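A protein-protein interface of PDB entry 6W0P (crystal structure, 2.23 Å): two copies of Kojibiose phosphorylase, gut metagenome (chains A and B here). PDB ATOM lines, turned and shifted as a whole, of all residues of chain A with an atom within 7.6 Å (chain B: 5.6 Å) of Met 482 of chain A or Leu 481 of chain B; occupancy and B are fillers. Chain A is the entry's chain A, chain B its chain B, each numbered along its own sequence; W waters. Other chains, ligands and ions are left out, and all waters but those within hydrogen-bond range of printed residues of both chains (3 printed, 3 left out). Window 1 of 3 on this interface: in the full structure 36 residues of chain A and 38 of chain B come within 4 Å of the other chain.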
ATOM      1  N   TRP A 410       7.544  12.479 -38.043  1.00  0.00           N
ATOM      2  CA  TRP A 410       8.507  13.386 -37.351  1.00  0.00           C
ATOM      3  C   TRP A 410       9.158  12.661 -36.152  1.00  0.00           C
ATOM      4  O   TRP A 410      10.362  12.874 -35.942  1.00  0.00           O
ATOM      5  CB  TRP A 410       7.829  14.699 -36.938  1.00  0.00           C
ATOM      6  CG  TRP A 410       6.904  14.545 -35.776  1.00  0.00           C
ATOM      7  CD1 TRP A 410       5.555  14.348 -35.822  1.00  0.00           C
ATOM      8  CD2 TRP A 410       7.266  14.556 -34.387  1.00  0.00           C
ATOM      9  NE1 TRP A 410       5.058  14.208 -34.558  1.00  0.00           N
ATOM     10  CE2 TRP A 410       6.087  14.311 -33.659  1.00  0.00           C
ATOM     11  CE3 TRP A 410       8.467  14.729 -33.694  1.00  0.00           C
ATOM     12  CZ2 TRP A 410       6.069  14.280 -32.270  1.00  0.00           C
ATOM     13  CZ3 TRP A 410       8.461  14.662 -32.320  1.00  0.00           C
ATOM     14  CH2 TRP A 410       7.272  14.439 -31.620  1.00  0.00           C
ATOM     15  N   GLN A 411       8.378  11.832 -35.437  1.00  0.00           N
ATOM     16  CA  GLN A 411       8.766  11.068 -34.224  1.00  0.00           C
ATOM     17  C   GLN A 411      10.032  10.246 -34.473  1.00  0.00           C
ATOM     18  O   GLN A 411      10.613   9.823 -33.468  1.00  0.00           O
ATOM     19  CB  GLN A 411       7.728  10.012 -33.807  1.00  0.00           C
ATOM     20  CG  GLN A 411       6.388  10.549 -33.365  1.00  0.00           C
ATOM     21  CD  GLN A 411       5.357  10.469 -34.471  1.00  0.00           C
ATOM     22  OE1 GLN A 411       5.611  10.881 -35.619  1.00  0.00           O
ATOM     23  NE2 GLN A 411       4.173   9.975 -34.113  1.00  0.00           N
ATOM     24  N   SER A 414      12.700  13.381 -37.204  1.00  0.00           N
ATOM     25  CA  SER A 414      13.225  14.596 -36.521  1.00  0.00           C
ATOM     26  C   SER A 414      14.084  14.201 -35.314  1.00  0.00           C
ATOM     27  O   SER A 414      14.770  15.093 -34.748  1.00  0.00           O
ATOM     28  CB  SER A 414      12.128  15.529 -36.105  1.00  0.00           C
ATOM     29  OG  SER A 414      11.397  15.978 -37.238  1.00  0.00           O
ATOM     30  N   THR A 415      14.086  12.924 -34.923  1.00  0.00           N
ATOM     31  CA  THR A 415      14.601  12.525 -33.587  1.00  0.00           C
ATOM     32  C   THR A 415      15.789  11.562 -33.641  1.00  0.00           C
ATOM     33  O   THR A 415      16.506  11.516 -32.614  1.00  0.00           O
ATOM     34  CB  THR A 415      13.478  11.925 -32.744  1.00  0.00           C
ATOM     35  OG1 THR A 415      13.022  10.754 -33.413  1.00  0.00           O
ATOM     36  CG2 THR A 415      12.363  12.916 -32.531  1.00  0.00           C
ATOM     37  N   ARG A 458      23.157  20.246 -34.227  1.00  0.00           N
ATOM     38  CA  ARG A 458      21.894  19.664 -33.705  1.00  0.00           C
ATOM     39  C   ARG A 458      22.121  19.335 -32.230  1.00  0.00           C
ATOM     40  O   ARG A 458      21.168  19.441 -31.418  1.00  0.00           O
ATOM     41  CB  ARG A 458      21.471  18.445 -34.535  1.00  0.00           C
ATOM     42  CG  ARG A 458      20.249  17.693 -34.003  1.00  0.00           C
ATOM     43  CD  ARG A 458      19.078  18.631 -33.758  1.00  0.00           C
ATOM     44  NE  ARG A 458      17.861  17.972 -33.303  1.00  0.00           N
ATOM     45  CZ  ARG A 458      17.620  17.553 -32.068  1.00  0.00           C
ATOM     46  NH1 ARG A 458      18.507  17.706 -31.100  1.00  0.00           N
ATOM     47  NH2 ARG A 458      16.460  16.997 -31.791  1.00  0.00           N
ATOM     48  N   TYR A 471      19.329  16.663 -27.270  1.00  0.00           N
ATOM     49  CA  TYR A 471      18.029  16.859 -26.595  1.00  0.00           C
ATOM     50  C   TYR A 471      16.940  16.536 -27.617  1.00  0.00           C
ATOM     51  O   TYR A 471      17.159  16.848 -28.797  1.00  0.00           O
ATOM     52  CB  TYR A 471      17.933  18.292 -26.061  1.00  0.00           C
ATOM     53  CG  TYR A 471      18.869  18.558 -24.918  1.00  0.00           C
ATOM     54  CD1 TYR A 471      20.162  18.999 -25.143  1.00  0.00           C
ATOM     55  CD2 TYR A 471      18.465  18.351 -23.618  1.00  0.00           C
ATOM     56  CE1 TYR A 471      21.040  19.236 -24.096  1.00  0.00           C
ATOM     57  CE2 TYR A 471      19.350  18.518 -22.564  1.00  0.00           C
ATOM     58  CZ  TYR A 471      20.641  18.963 -22.805  1.00  0.00           C
ATOM     59  OH  TYR A 471      21.492  19.160 -21.762  1.00  0.00           O
ATOM     60  N   GLY A 472      15.832  15.933 -27.162  1.00  0.00           N
ATOM     61  CA  GLY A 472      14.617  15.697 -27.956  1.00  0.00           C
ATOM     62  C   GLY A 472      14.896  14.680 -29.029  1.00  0.00           C
ATOM     63  O   GLY A 472      14.659  14.975 -30.204  1.00  0.00           O
ATOM     64  N   VAL A 473      15.458  13.539 -28.634  1.00  0.00           N
ATOM     65  CA  VAL A 473      15.965  12.516 -29.589  1.00  0.00           C
ATOM     66  C   VAL A 473      15.297  11.171 -29.330  1.00  0.00           C
ATOM     67  O   VAL A 473      14.486  11.034 -28.368  1.00  0.00           O
ATOM     68  CB  VAL A 473      17.499  12.419 -29.554  1.00  0.00           C
ATOM     69  CG1 VAL A 473      18.123  13.717 -30.049  1.00  0.00           C
ATOM     70  CG2 VAL A 473      18.046  12.019 -28.191  1.00  0.00           C
ATOM     71  N   MET A 474      15.630  10.233 -30.202  1.00  0.00           N
ATOM     72  CA  MET A 474      15.249   8.818 -30.111  1.00  0.00           C
ATOM     73  C   MET A 474      16.449   8.006 -30.590  1.00  0.00           C
ATOM     74  O   MET A 474      16.975   8.328 -31.688  1.00  0.00           O
ATOM     75  CB  MET A 474      14.034   8.544 -31.007  1.00  0.00           C
ATOM     76  CG  MET A 474      13.715   7.078 -31.151  1.00  0.00           C
ATOM     77  SD  MET A 474      12.348   6.714 -32.287  1.00  0.00           S
ATOM     78  CE  MET A 474      10.940   7.265 -31.333  1.00  0.00           C
ATOM     79  N   GLY A 475      16.851   7.000 -29.806  1.00  0.00           N
ATOM     80  CA  GLY A 475      17.919   6.066 -30.175  1.00  0.00           C
ATOM     81  C   GLY A 475      17.340   4.960 -31.037  1.00  0.00           C
ATOM     82  O   GLY A 475      16.195   5.050 -31.474  1.00  0.00           O
ATOM     83  N   LYS A 480      11.379   4.945 -26.943  1.00  0.00           N
ATOM     84  CA  LYS A 480      11.813   6.124 -26.139  1.00  0.00           C
ATOM     85  C   LYS A 480      11.895   7.360 -27.040  1.00  0.00           C
ATOM     86  O   LYS A 480      12.851   7.435 -27.864  1.00  0.00           O
ATOM     87  CB  LYS A 480      13.134   5.837 -25.427  1.00  0.00           C
ATOM     88  CG  LYS A 480      12.960   5.043 -24.147  1.00  0.00           C
ATOM     89  CD  LYS A 480      12.234   5.823 -23.062  1.00  0.00           C
ATOM     90  CE  LYS A 480      11.510   4.930 -22.083  1.00  0.00           C
ATOM     91  NZ  LYS A 480      10.628   3.951 -22.768  1.00  0.00           N
ATOM     92  N   LEU A 481      10.954   8.284 -26.849  1.00  0.00           N
ATOM     93  CA  LEU A 481      10.700   9.458 -27.732  1.00  0.00           C
ATOM     94  C   LEU A 481      10.906  10.786 -26.985  1.00  0.00           C
ATOM     95  O   LEU A 481      10.324  10.969 -25.915  1.00  0.00           O
ATOM     96  CB  LEU A 481       9.276   9.339 -28.284  1.00  0.00           C
ATOM     97  CG  LEU A 481       8.728  10.580 -28.991  1.00  0.00           C
ATOM     98  CD1 LEU A 481       9.617  11.002 -30.153  1.00  0.00           C
ATOM     99  CD2 LEU A 481       7.302  10.346 -29.458  1.00  0.00           C
ATOM    100  N   MET A 482      11.697  11.695 -27.560  1.00  0.00           N
ATOM    101  CA  MET A 482      11.941  13.065 -27.032  1.00  0.00           C
ATOM    102  C   MET A 482      12.614  12.904 -25.670  1.00  0.00           C
ATOM    103  O   MET A 482      12.251  13.609 -24.688  1.00  0.00           O
ATOM    104  CB  MET A 482      10.656  13.891 -26.886  1.00  0.00           C
ATOM    105  CG  MET A 482       9.948  14.213 -28.205  1.00  0.00           C
ATOM    106  SD  MET A 482      10.894  15.237 -29.334  1.00  0.00           S
ATOM    107  CE  MET A 482      11.361  16.603 -28.263  1.00  0.00           C
ATOM    108  N   VAL A 483      13.548  11.962 -25.599  1.00  0.00           N
ATOM    109  CA  VAL A 483      14.399  11.802 -24.395  1.00  0.00           C
ATOM    110  C   VAL A 483      15.658  12.638 -24.584  1.00  0.00           C
ATOM    111  O   VAL A 483      15.934  13.055 -25.720  1.00  0.00           O
ATOM    112  CB  VAL A 483      14.722  10.327 -24.116  1.00  0.00           C
ATOM    113  CG1 VAL A 483      13.453   9.570 -23.788  1.00  0.00           C
ATOM    114  CG2 VAL A 483      15.504   9.665 -25.236  1.00  0.00           C
ATOM    115  N   ASN A 484      16.393  12.826 -23.497  1.00  0.00           N
ATOM    116  CA  ASN A 484      17.684  13.538 -23.463  1.00  0.00           C
ATOM    117  C   ASN A 484      18.774  12.571 -23.012  1.00  0.00           C
ATOM    118  O   ASN A 484      18.468  11.676 -22.250  1.00  0.00           O
ATOM    119  CB  ASN A 484      17.603  14.744 -22.540  1.00  0.00           C
ATOM    120  CG  ASN A 484      16.412  15.624 -22.828  1.00  0.00           C
ATOM    121  OD1 ASN A 484      16.126  15.931 -23.980  1.00  0.00           O
ATOM    122  ND2 ASN A 484      15.759  16.081 -21.780  1.00  0.00           N
ATOM    123  N   ASN A 549      18.888   6.300 -21.456  1.00  0.00           N
ATOM    124  CA  ASN A 549      18.645   7.762 -21.562  1.00  0.00           C
ATOM    125  C   ASN A 549      18.421   8.314 -20.148  1.00  0.00           C
ATOM    126  O   ASN A 549      18.234   7.500 -19.208  1.00  0.00           O
ATOM    127  CB  ASN A 549      17.510   8.080 -22.543  1.00  0.00           C
ATOM    128  CG  ASN A 549      16.173   7.508 -22.123  1.00  0.00           C
ATOM    129  OD1 ASN A 549      15.656   6.605 -22.790  1.00  0.00           O
ATOM    130  ND2 ASN A 549      15.595   8.051 -21.057  1.00  0.00           N
ATOM    131  N   TYR A 580       5.599   4.071 -24.682  1.00  0.00           N
ATOM    132  CA  TYR A 580       6.717   5.024 -24.448  1.00  0.00           C
ATOM    133  C   TYR A 580       7.011   5.194 -22.956  1.00  0.00           C
ATOM    134  O   TYR A 580       8.167   5.540 -22.612  1.00  0.00           O
ATOM    135  CB  TYR A 580       6.427   6.385 -25.074  1.00  0.00           C
ATOM    136  CG  TYR A 580       6.417   6.370 -26.578  1.00  0.00           C
ATOM    137  CD1 TYR A 580       7.578   6.151 -27.290  1.00  0.00           C
ATOM    138  CD2 TYR A 580       5.265   6.635 -27.286  1.00  0.00           C
ATOM    139  CE1 TYR A 580       7.593   6.168 -28.670  1.00  0.00           C
ATOM    140  CE2 TYR A 580       5.258   6.667 -28.670  1.00  0.00           C
ATOM    141  CZ  TYR A 580       6.426   6.425 -29.365  1.00  0.00           C
ATOM    142  OH  TYR A 580       6.419   6.404 -30.726  1.00  0.00           O
ATOM    143  N   TRP B 410      -2.171  13.442 -31.239  1.00  0.00           N
ATOM    144  CA  TRP B 410      -1.813  12.594 -30.078  1.00  0.00           C
ATOM    145  C   TRP B 410      -0.880  13.388 -29.145  1.00  0.00           C
ATOM    146  O   TRP B 410      -0.987  13.193 -27.928  1.00  0.00           O
ATOM    147  CB  TRP B 410      -1.223  11.261 -30.532  1.00  0.00           C
ATOM    148  CG  TRP B 410       0.173  11.411 -31.045  1.00  0.00           C
ATOM    149  CD1 TRP B 410       0.544  11.624 -32.339  1.00  0.00           C
ATOM    150  CD2 TRP B 410       1.374  11.457 -30.255  1.00  0.00           C
ATOM    151  NE1 TRP B 410       1.901  11.755 -32.411  1.00  0.00           N
ATOM    152  CE2 TRP B 410       2.439  11.668 -31.153  1.00  0.00           C
ATOM    153  CE3 TRP B 410       1.657  11.331 -28.888  1.00  0.00           C
ATOM    154  CZ2 TRP B 410       3.768  11.757 -30.727  1.00  0.00           C
ATOM    155  CZ3 TRP B 410       2.967  11.413 -28.465  1.00  0.00           C
ATOM    156  CH2 TRP B 410       4.008  11.615 -29.378  1.00  0.00           C
ATOM    157  N   GLN B 411      -0.042  14.283 -29.689  1.00  0.00           N
ATOM    158  CA  GLN B 411       0.914  15.114 -28.913  1.00  0.00           C
ATOM    159  C   GLN B 411       0.194  15.867 -27.794  1.00  0.00           C
ATOM    160  O   GLN B 411       0.871  16.167 -26.795  1.00  0.00           O
ATOM    161  CB  GLN B 411       1.589  16.213 -29.731  1.00  0.00           C
ATOM    162  CG  GLN B 411       2.476  15.710 -30.833  1.00  0.00           C
ATOM    163  CD  GLN B 411       1.762  15.627 -32.166  1.00  0.00           C
ATOM    164  OE1 GLN B 411       0.697  15.011 -32.308  1.00  0.00           O
ATOM    165  NE2 GLN B 411       2.405  16.185 -33.175  1.00  0.00           N
ATOM    166  N   HIS B 412      -1.060  16.260 -27.997  1.00  0.00           N
ATOM    167  CA  HIS B 412      -1.890  16.959 -26.987  1.00  0.00           C
ATOM    168  C   HIS B 412      -2.924  15.995 -26.366  1.00  0.00           C
ATOM    169  O   HIS B 412      -3.042  15.951 -25.119  1.00  0.00           O
ATOM    170  CB  HIS B 412      -2.515  18.219 -27.598  1.00  0.00           C
ATOM    171  CG  HIS B 412      -1.536  19.197 -28.164  1.00  0.00           C
ATOM    172  ND1 HIS B 412      -1.914  20.188 -29.040  1.00  0.00           N
ATOM    173  CD2 HIS B 412      -0.200  19.317 -28.041  1.00  0.00           C
ATOM    174  CE1 HIS B 412      -0.862  20.888 -29.409  1.00  0.00           C
ATOM    175  NE2 HIS B 412       0.200  20.374 -28.815  1.00  0.00           N
ATOM    176  N   THR B 415      -1.565  13.211 -23.983  1.00  0.00           N
ATOM    177  CA  THR B 415      -0.522  13.676 -23.032  1.00  0.00           C
ATOM    178  C   THR B 415      -1.015  14.706 -22.018  1.00  0.00           C
ATOM    179  O   THR B 415      -0.311  14.861 -21.005  1.00  0.00           O
ATOM    180  CB  THR B 415       0.638  14.295 -23.823  1.00  0.00           C
ATOM    181  OG1 THR B 415       0.175  15.513 -24.413  1.00  0.00           O
ATOM    182  CG2 THR B 415       1.125  13.367 -24.904  1.00  0.00           C
ATOM    183  N   VAL B 473       3.866  13.040 -20.535  1.00  0.00           N
ATOM    184  CA  VAL B 473       2.773  14.041 -20.431  1.00  0.00           C
ATOM    185  C   VAL B 473       3.231  15.379 -21.008  1.00  0.00           C
ATOM    186  O   VAL B 473       4.440  15.545 -21.320  1.00  0.00           O
ATOM    187  CB  VAL B 473       2.276  14.174 -18.981  1.00  0.00           C
ATOM    188  CG1 VAL B 473       1.707  12.864 -18.477  1.00  0.00           C
ATOM    189  CG2 VAL B 473       3.367  14.648 -18.051  1.00  0.00           C
ATOM    190  N   MET B 474       2.254  16.269 -21.152  1.00  0.00           N
ATOM    191  CA  MET B 474       2.431  17.706 -21.450  1.00  0.00           C
ATOM    192  C   MET B 474       1.503  18.484 -20.517  1.00  0.00           C
ATOM    193  O   MET B 474       0.322  18.066 -20.334  1.00  0.00           O
ATOM    194  CB  MET B 474       2.058  17.979 -22.908  1.00  0.00           C
ATOM    195  CG  MET B 474       1.948  19.424 -23.284  1.00  0.00           C
ATOM    196  SD  MET B 474       1.342  19.552 -24.972  1.00  0.00           S
ATOM    197  CE  MET B 474       2.775  18.904 -25.834  1.00  0.00           C
ATOM    198  N   GLU B 478       2.827  23.777 -23.968  1.00  0.00           N
ATOM    199  CA  GLU B 478       2.824  22.789 -25.078  1.00  0.00           C
ATOM    200  C   GLU B 478       4.215  22.723 -25.734  1.00  0.00           C
ATOM    201  O   GLU B 478       4.354  21.983 -26.708  1.00  0.00           O
ATOM    202  CB  GLU B 478       1.745  23.147 -26.110  1.00  0.00           C
ATOM    203  CG  GLU B 478       0.338  23.188 -25.524  1.00  0.00           C
ATOM    204  CD  GLU B 478      -0.789  23.608 -26.452  1.00  0.00           C
ATOM    205  OE1 GLU B 478      -0.543  23.866 -27.652  1.00  0.00           O
ATOM    206  OE2 GLU B 478      -1.919  23.680 -25.958  1.00  0.00           O
ATOM    207  N   PHE B 479       5.228  23.438 -25.232  1.00  0.00           N
ATOM    208  CA  PHE B 479       6.621  23.324 -25.741  1.00  0.00           C
ATOM    209  C   PHE B 479       7.386  22.234 -24.981  1.00  0.00           C
ATOM    210  O   PHE B 479       8.606  22.135 -25.147  1.00  0.00           O
ATOM    211  CB  PHE B 479       7.325  24.682 -25.697  1.00  0.00           C
ATOM    212  CG  PHE B 479       6.692  25.764 -26.541  1.00  0.00           C
ATOM    213  CD1 PHE B 479       5.825  25.464 -27.587  1.00  0.00           C
ATOM    214  CD2 PHE B 479       7.033  27.094 -26.342  1.00  0.00           C
ATOM    215  CE1 PHE B 479       5.251  26.466 -28.356  1.00  0.00           C
ATOM    216  CE2 PHE B 479       6.471  28.089 -27.127  1.00  0.00           C
ATOM    217  CZ  PHE B 479       5.592  27.781 -28.138  1.00  0.00           C
ATOM    218  N   LYS B 480       6.700  21.425 -24.180  1.00  0.00           N
ATOM    219  CA  LYS B 480       7.284  20.266 -23.444  1.00  0.00           C
ATOM    220  C   LYS B 480       6.363  19.060 -23.652  1.00  0.00           C
ATOM    221  O   LYS B 480       5.231  19.095 -23.180  1.00  0.00           O
ATOM    222  CB  LYS B 480       7.493  20.599 -21.963  1.00  0.00           C
ATOM    223  CG  LYS B 480       8.669  21.523 -21.690  1.00  0.00           C
ATOM    224  CD  LYS B 480      10.003  20.830 -21.918  1.00  0.00           C
ATOM    225  CE  LYS B 480      11.136  21.781 -22.222  1.00  0.00           C
ATOM    226  NZ  LYS B 480      10.902  22.507 -23.488  1.00  0.00           N
ATOM    227  N   LEU B 481       6.870  18.056 -24.369  1.00  0.00           N
ATOM    228  CA  LEU B 481       6.148  16.863 -24.869  1.00  0.00           C
ATOM    229  C   LEU B 481       6.843  15.589 -24.350  1.00  0.00           C
ATOM    230  O   LEU B 481       8.063  15.472 -24.525  1.00  0.00           O
ATOM    231  CB  LEU B 481       6.163  16.950 -26.401  1.00  0.00           C
ATOM    232  CG  LEU B 481       5.685  15.702 -27.138  1.00  0.00           C
ATOM    233  CD1 LEU B 481       4.270  15.336 -26.719  1.00  0.00           C
ATOM    234  CD2 LEU B 481       5.756  15.895 -28.633  1.00  0.00           C
ATOM    235  N   MET B 482       6.084  14.680 -23.720  1.00  0.00           N
ATOM    236  CA  MET B 482       6.558  13.350 -23.255  1.00  0.00           C
ATOM    237  C   MET B 482       7.590  13.543 -22.147  1.00  0.00           C
ATOM    238  O   MET B 482       8.498  12.696 -22.042  1.00  0.00           O
ATOM    239  CB  MET B 482       7.200  12.521 -24.374  1.00  0.00           C
ATOM    240  CG  MET B 482       6.267  12.252 -25.557  1.00  0.00           C
ATOM    241  SD  MET B 482       5.094  10.937 -25.211  1.00  0.00           S
ATOM    242  CE  MET B 482       3.810  11.879 -24.419  1.00  0.00           C
ATOM    243  N   VAL B 483       7.401  14.573 -21.323  1.00  0.00           N
ATOM    244  CA  VAL B 483       8.191  14.798 -20.075  1.00  0.00           C
ATOM    245  C   VAL B 483       7.569  13.969 -18.948  1.00  0.00           C
ATOM    246  O   VAL B 483       6.468  13.421 -19.118  1.00  0.00           O
ATOM    247  CB  VAL B 483       8.245  16.293 -19.718  1.00  0.00           C
ATOM    248  CG1 VAL B 483       9.053  17.063 -20.745  1.00  0.00           C
ATOM    249  CG2 VAL B 483       6.846  16.893 -19.569  1.00  0.00           C
ATOM    250  N   TYR B 576       9.813  21.771 -36.720  1.00  0.00           N
ATOM    251  CA  TYR B 576       8.750  21.374 -35.764  1.00  0.00           C
ATOM    252  C   TYR B 576       9.340  21.039 -34.401  1.00  0.00           C
ATOM    253  O   TYR B 576       8.780  21.517 -33.409  1.00  0.00           O
ATOM    254  CB  TYR B 576       7.962  20.150 -36.239  1.00  0.00           C
ATOM    255  CG  TYR B 576       6.967  19.642 -35.214  1.00  0.00           C
ATOM    256  CD1 TYR B 576       5.928  20.448 -34.769  1.00  0.00           C
ATOM    257  CD2 TYR B 576       7.086  18.381 -34.655  1.00  0.00           C
ATOM    258  CE1 TYR B 576       5.030  20.016 -33.812  1.00  0.00           C
ATOM    259  CE2 TYR B 576       6.207  17.940 -33.681  1.00  0.00           C
ATOM    260  CZ  TYR B 576       5.180  18.762 -33.261  1.00  0.00           C
ATOM    261  OH  TYR B 576       4.314  18.329 -32.316  1.00  0.00           O
ATOM    262  N   ASP B 577      10.409  20.236 -34.374  1.00  0.00           N
ATOM    263  CA  ASP B 577      10.959  19.604 -33.149  1.00  0.00           C
ATOM    264  C   ASP B 577      11.720  20.640 -32.294  1.00  0.00           C
ATOM    265  O   ASP B 577      11.843  20.427 -31.091  1.00  0.00           O
ATOM    266  CB  ASP B 577      11.833  18.402 -33.539  1.00  0.00           C
ATOM    267  CG  ASP B 577      13.259  18.758 -33.957  1.00  0.00           C
ATOM    268  OD1 ASP B 577      13.501  19.008 -35.168  1.00  0.00           O
ATOM    269  OD2 ASP B 577      14.107  18.845 -33.051  1.00  0.00           O
ATOM    270  N   TYR B 580      10.762  22.313 -28.715  1.00  0.00           N
ATOM    271  CA  TYR B 580      10.670  21.381 -27.559  1.00  0.00           C
ATOM    272  C   TYR B 580      11.991  21.298 -26.802  1.00  0.00           C
ATOM    273  O   TYR B 580      11.909  21.042 -25.608  1.00  0.00           O
ATOM    274  CB  TYR B 580      10.257  19.971 -27.979  1.00  0.00           C
ATOM    275  CG  TYR B 580       8.866  19.889 -28.556  1.00  0.00           C
ATOM    276  CD1 TYR B 580       7.741  20.105 -27.772  1.00  0.00           C
ATOM    277  CD2 TYR B 580       8.678  19.637 -29.900  1.00  0.00           C
ATOM    278  CE1 TYR B 580       6.461  20.024 -28.298  1.00  0.00           C
ATOM    279  CE2 TYR B 580       7.406  19.552 -30.442  1.00  0.00           C
ATOM    280  CZ  TYR B 580       6.291  19.723 -29.634  1.00  0.00           C
ATOM    281  OH  TYR B 580       5.044  19.658 -30.196  1.00  0.00           O
ATOM    282  N   ARG B 581      13.139  21.567 -27.439  1.00  0.00           N
ATOM    283  CA  ARG B 581      14.456  21.199 -26.852  1.00  0.00           C
ATOM    284  C   ARG B 581      15.194  22.455 -26.401  1.00  0.00           C
ATOM    285  O   ARG B 581      16.424  22.519 -26.588  1.00  0.00           O
ATOM    286  CB  ARG B 581      15.247  20.308 -27.813  1.00  0.00           C
ATOM    287  CG  ARG B 581      15.486  20.869 -29.201  1.00  0.00           C
ATOM    288  CD  ARG B 581      16.107  19.777 -30.061  1.00  0.00           C
ATOM    289  NE  ARG B 581      16.165  20.228 -31.448  1.00  0.00           N
ATOM    290  CZ  ARG B 581      17.090  21.055 -31.929  1.00  0.00           C
ATOM    291  NH1 ARG B 581      18.056  21.503 -31.144  1.00  0.00           N
ATOM    292  NH2 ARG B 581      17.062  21.406 -33.202  1.00  0.00           N
HETATM  293  O   HOH W   1      11.644  18.807 -36.791  1.00  0.00           O
HETATM  294  O   HOH W   2       2.392  12.975 -34.875  1.00  0.00           O
HETATM  295  O   HOH W   3      15.898  17.532 -35.305  1.00  0.00           O
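The backbone carbonyl oxygen of Val 473 of chain A lies within hydrogen-bond range of the backbone NH of Met 482 of chain A, 3.0 Å away.
The backbone carbonyl oxygen (O) of Val 473 of chain B is in hydrogen-bond range of the backbone NH (N) of Met 482 of chain B (3.0 Å).
O of Gln 411 of chain B sits at hydrogen-bond distance from OG1 of Thr 415 of chain B, at 2.6 Å.
The side-chain amide oxygen (OE1) of Gln 411 of chain B sits close to the indole nitrogen (NE1) of Trp 410 of chain B, at 3.5 Å.
O of Gly 472 of chain A is in hydrogen-bond range of NH2 of Arg 458 of chain A.
The guanidinium group of Arg 458 of chain A sits close to the guanidinium group of Arg 581 of chain B (3.3 Å).
The indole nitrogen of Trp 410 of chain B lies close to the side-chain amide nitrogen of Gln 411 of chain A (3.4 Å).
The guanidinium group of Arg 458 of chain A lies within salt-bridge range of the side-chain carboxylate of Asp 577 of chain B, 3.2 Å away.
Printed residues of chain B within 4 Å of Leu 481 of chain A: Trp 410 and Met 482.
Lys 480 of chain B touches none of the printed residues of chain A.
Leu 481 of chain B touches just these residues of chain A: Trp 410 and Met 482.
Of the printed residues of chain A, Met 482 of chain B touches Leu 481.
The nearest residue of chain B that does not touch Met 482 of chain A is Met 482 of chain B (4.5 Å).
The nearest residue of chain A that does not touch Leu 481 of chain B is Leu 481 of chain A (5.2 Å).
The nearest printed residue of chain B that does not touch Arg 458 of chain A is Tyr 580 of chain B (7.9 Å).
Of the 16 printed residues of chain B, 8 touch a printed residue of chain A.
Printed residues of chain B that touch a printed residue of chain A: Trp 410, Gln 411, Leu 481, Met 482, Tyr 576, Asp 577, Tyr 580 and Arg 581.
Hydrophobic or aromatic side chains of chain B that line the printed part of chain A: Trp 410, Leu 481, Met 482, Tyr 576 and Tyr 580.
Of the 17 printed residues of chain A, 7 touch a printed residue of chain B.
Printed residues of chain A that touch a printed residue of chain B: Trp 410, Gln 411, Ser 414, Arg 458, Tyr 471, Leu 481 and Met 482.
Along chain A the printed residues that touch a printed residue of chain B span positions 410 to 482.
Among the printed residues, Asp or Glu carboxylates within 4 Å of a Lys or Arg side-chain nitrogen of the other chain: Arg 458 of chain A with Asp 577 of chain B.
Water W1 lies within hydrogen-bond range of the side-chain carboxylate of Asp 577 of chain B (2.5 Å), the side-chain hydroxyl of Ser 414 of chain A (2.9 Å) and the backbone NH of Tyr 576 of chain B (3.5 Å).
Water W3 lies within hydrogen-bond range of the backbone carbonyl oxygen of Ser 414 of chain A, the side-chain carboxylate of Asp 577 of chain B and the guanidinium group of Arg 458 of chain A.
Water W2 bridges NE1 of Trp 410 of chain B (2.8 Å) and NE1 of Trp 410 of chain A (3.0 Å).
Trp 410 of chain B touches Trp 410 of chain A.
Trp 410 of chain A touches Gln 411 of chain B (NE1 to NE2, 3.6 Å).
CH2 of Trp 410 of chain A touches CD2 of Leu 481 of chain B, 3.7 Å away.
Trp 410 of chain A touches Tyr 576 of chain B (CD2 to CE2, 3.6 Å).
CB of Ser 414 of chain A touches OD1 of Asp 577 of chain B, 3.9 Å away.
O of Tyr 471 of chain A touches CD of Arg 581 of chain B, at 3.4 Å.
CD2 of Leu 481 of chain A touches CH2 of Trp 410 of chain B (3.5 Å).
O of Leu 481 of chain A touches CB of Met 482 of chain B, 3.8 Å away.
Leu 481 of chain B touches Met 482 of chain A.
Met 482 of chain A touches Tyr 580 of chain B (CE to CB, 3.6 Å).
Trp 410 of chain A touches its own counterpart, Trp 410 of chain B.
Trp 410 of chain A touches Gln 411 of chain B, and with the chains exchanged Gln 411 of chain A touches Trp 410 of chain B.
Trp 410 of chain A touches Leu 481 of chain B, and with the chains exchanged Leu 481 of chain A touches Trp 410 of chain B.
Leu 481 of chain A touches Met 482 of chain B, and with the chains exchanged Met 482 of chain A touches Leu 481 of chain B.
Positions printed for both chains: 410, 411, 415, 473, 474, 480, 481, 482, 483 and 580.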
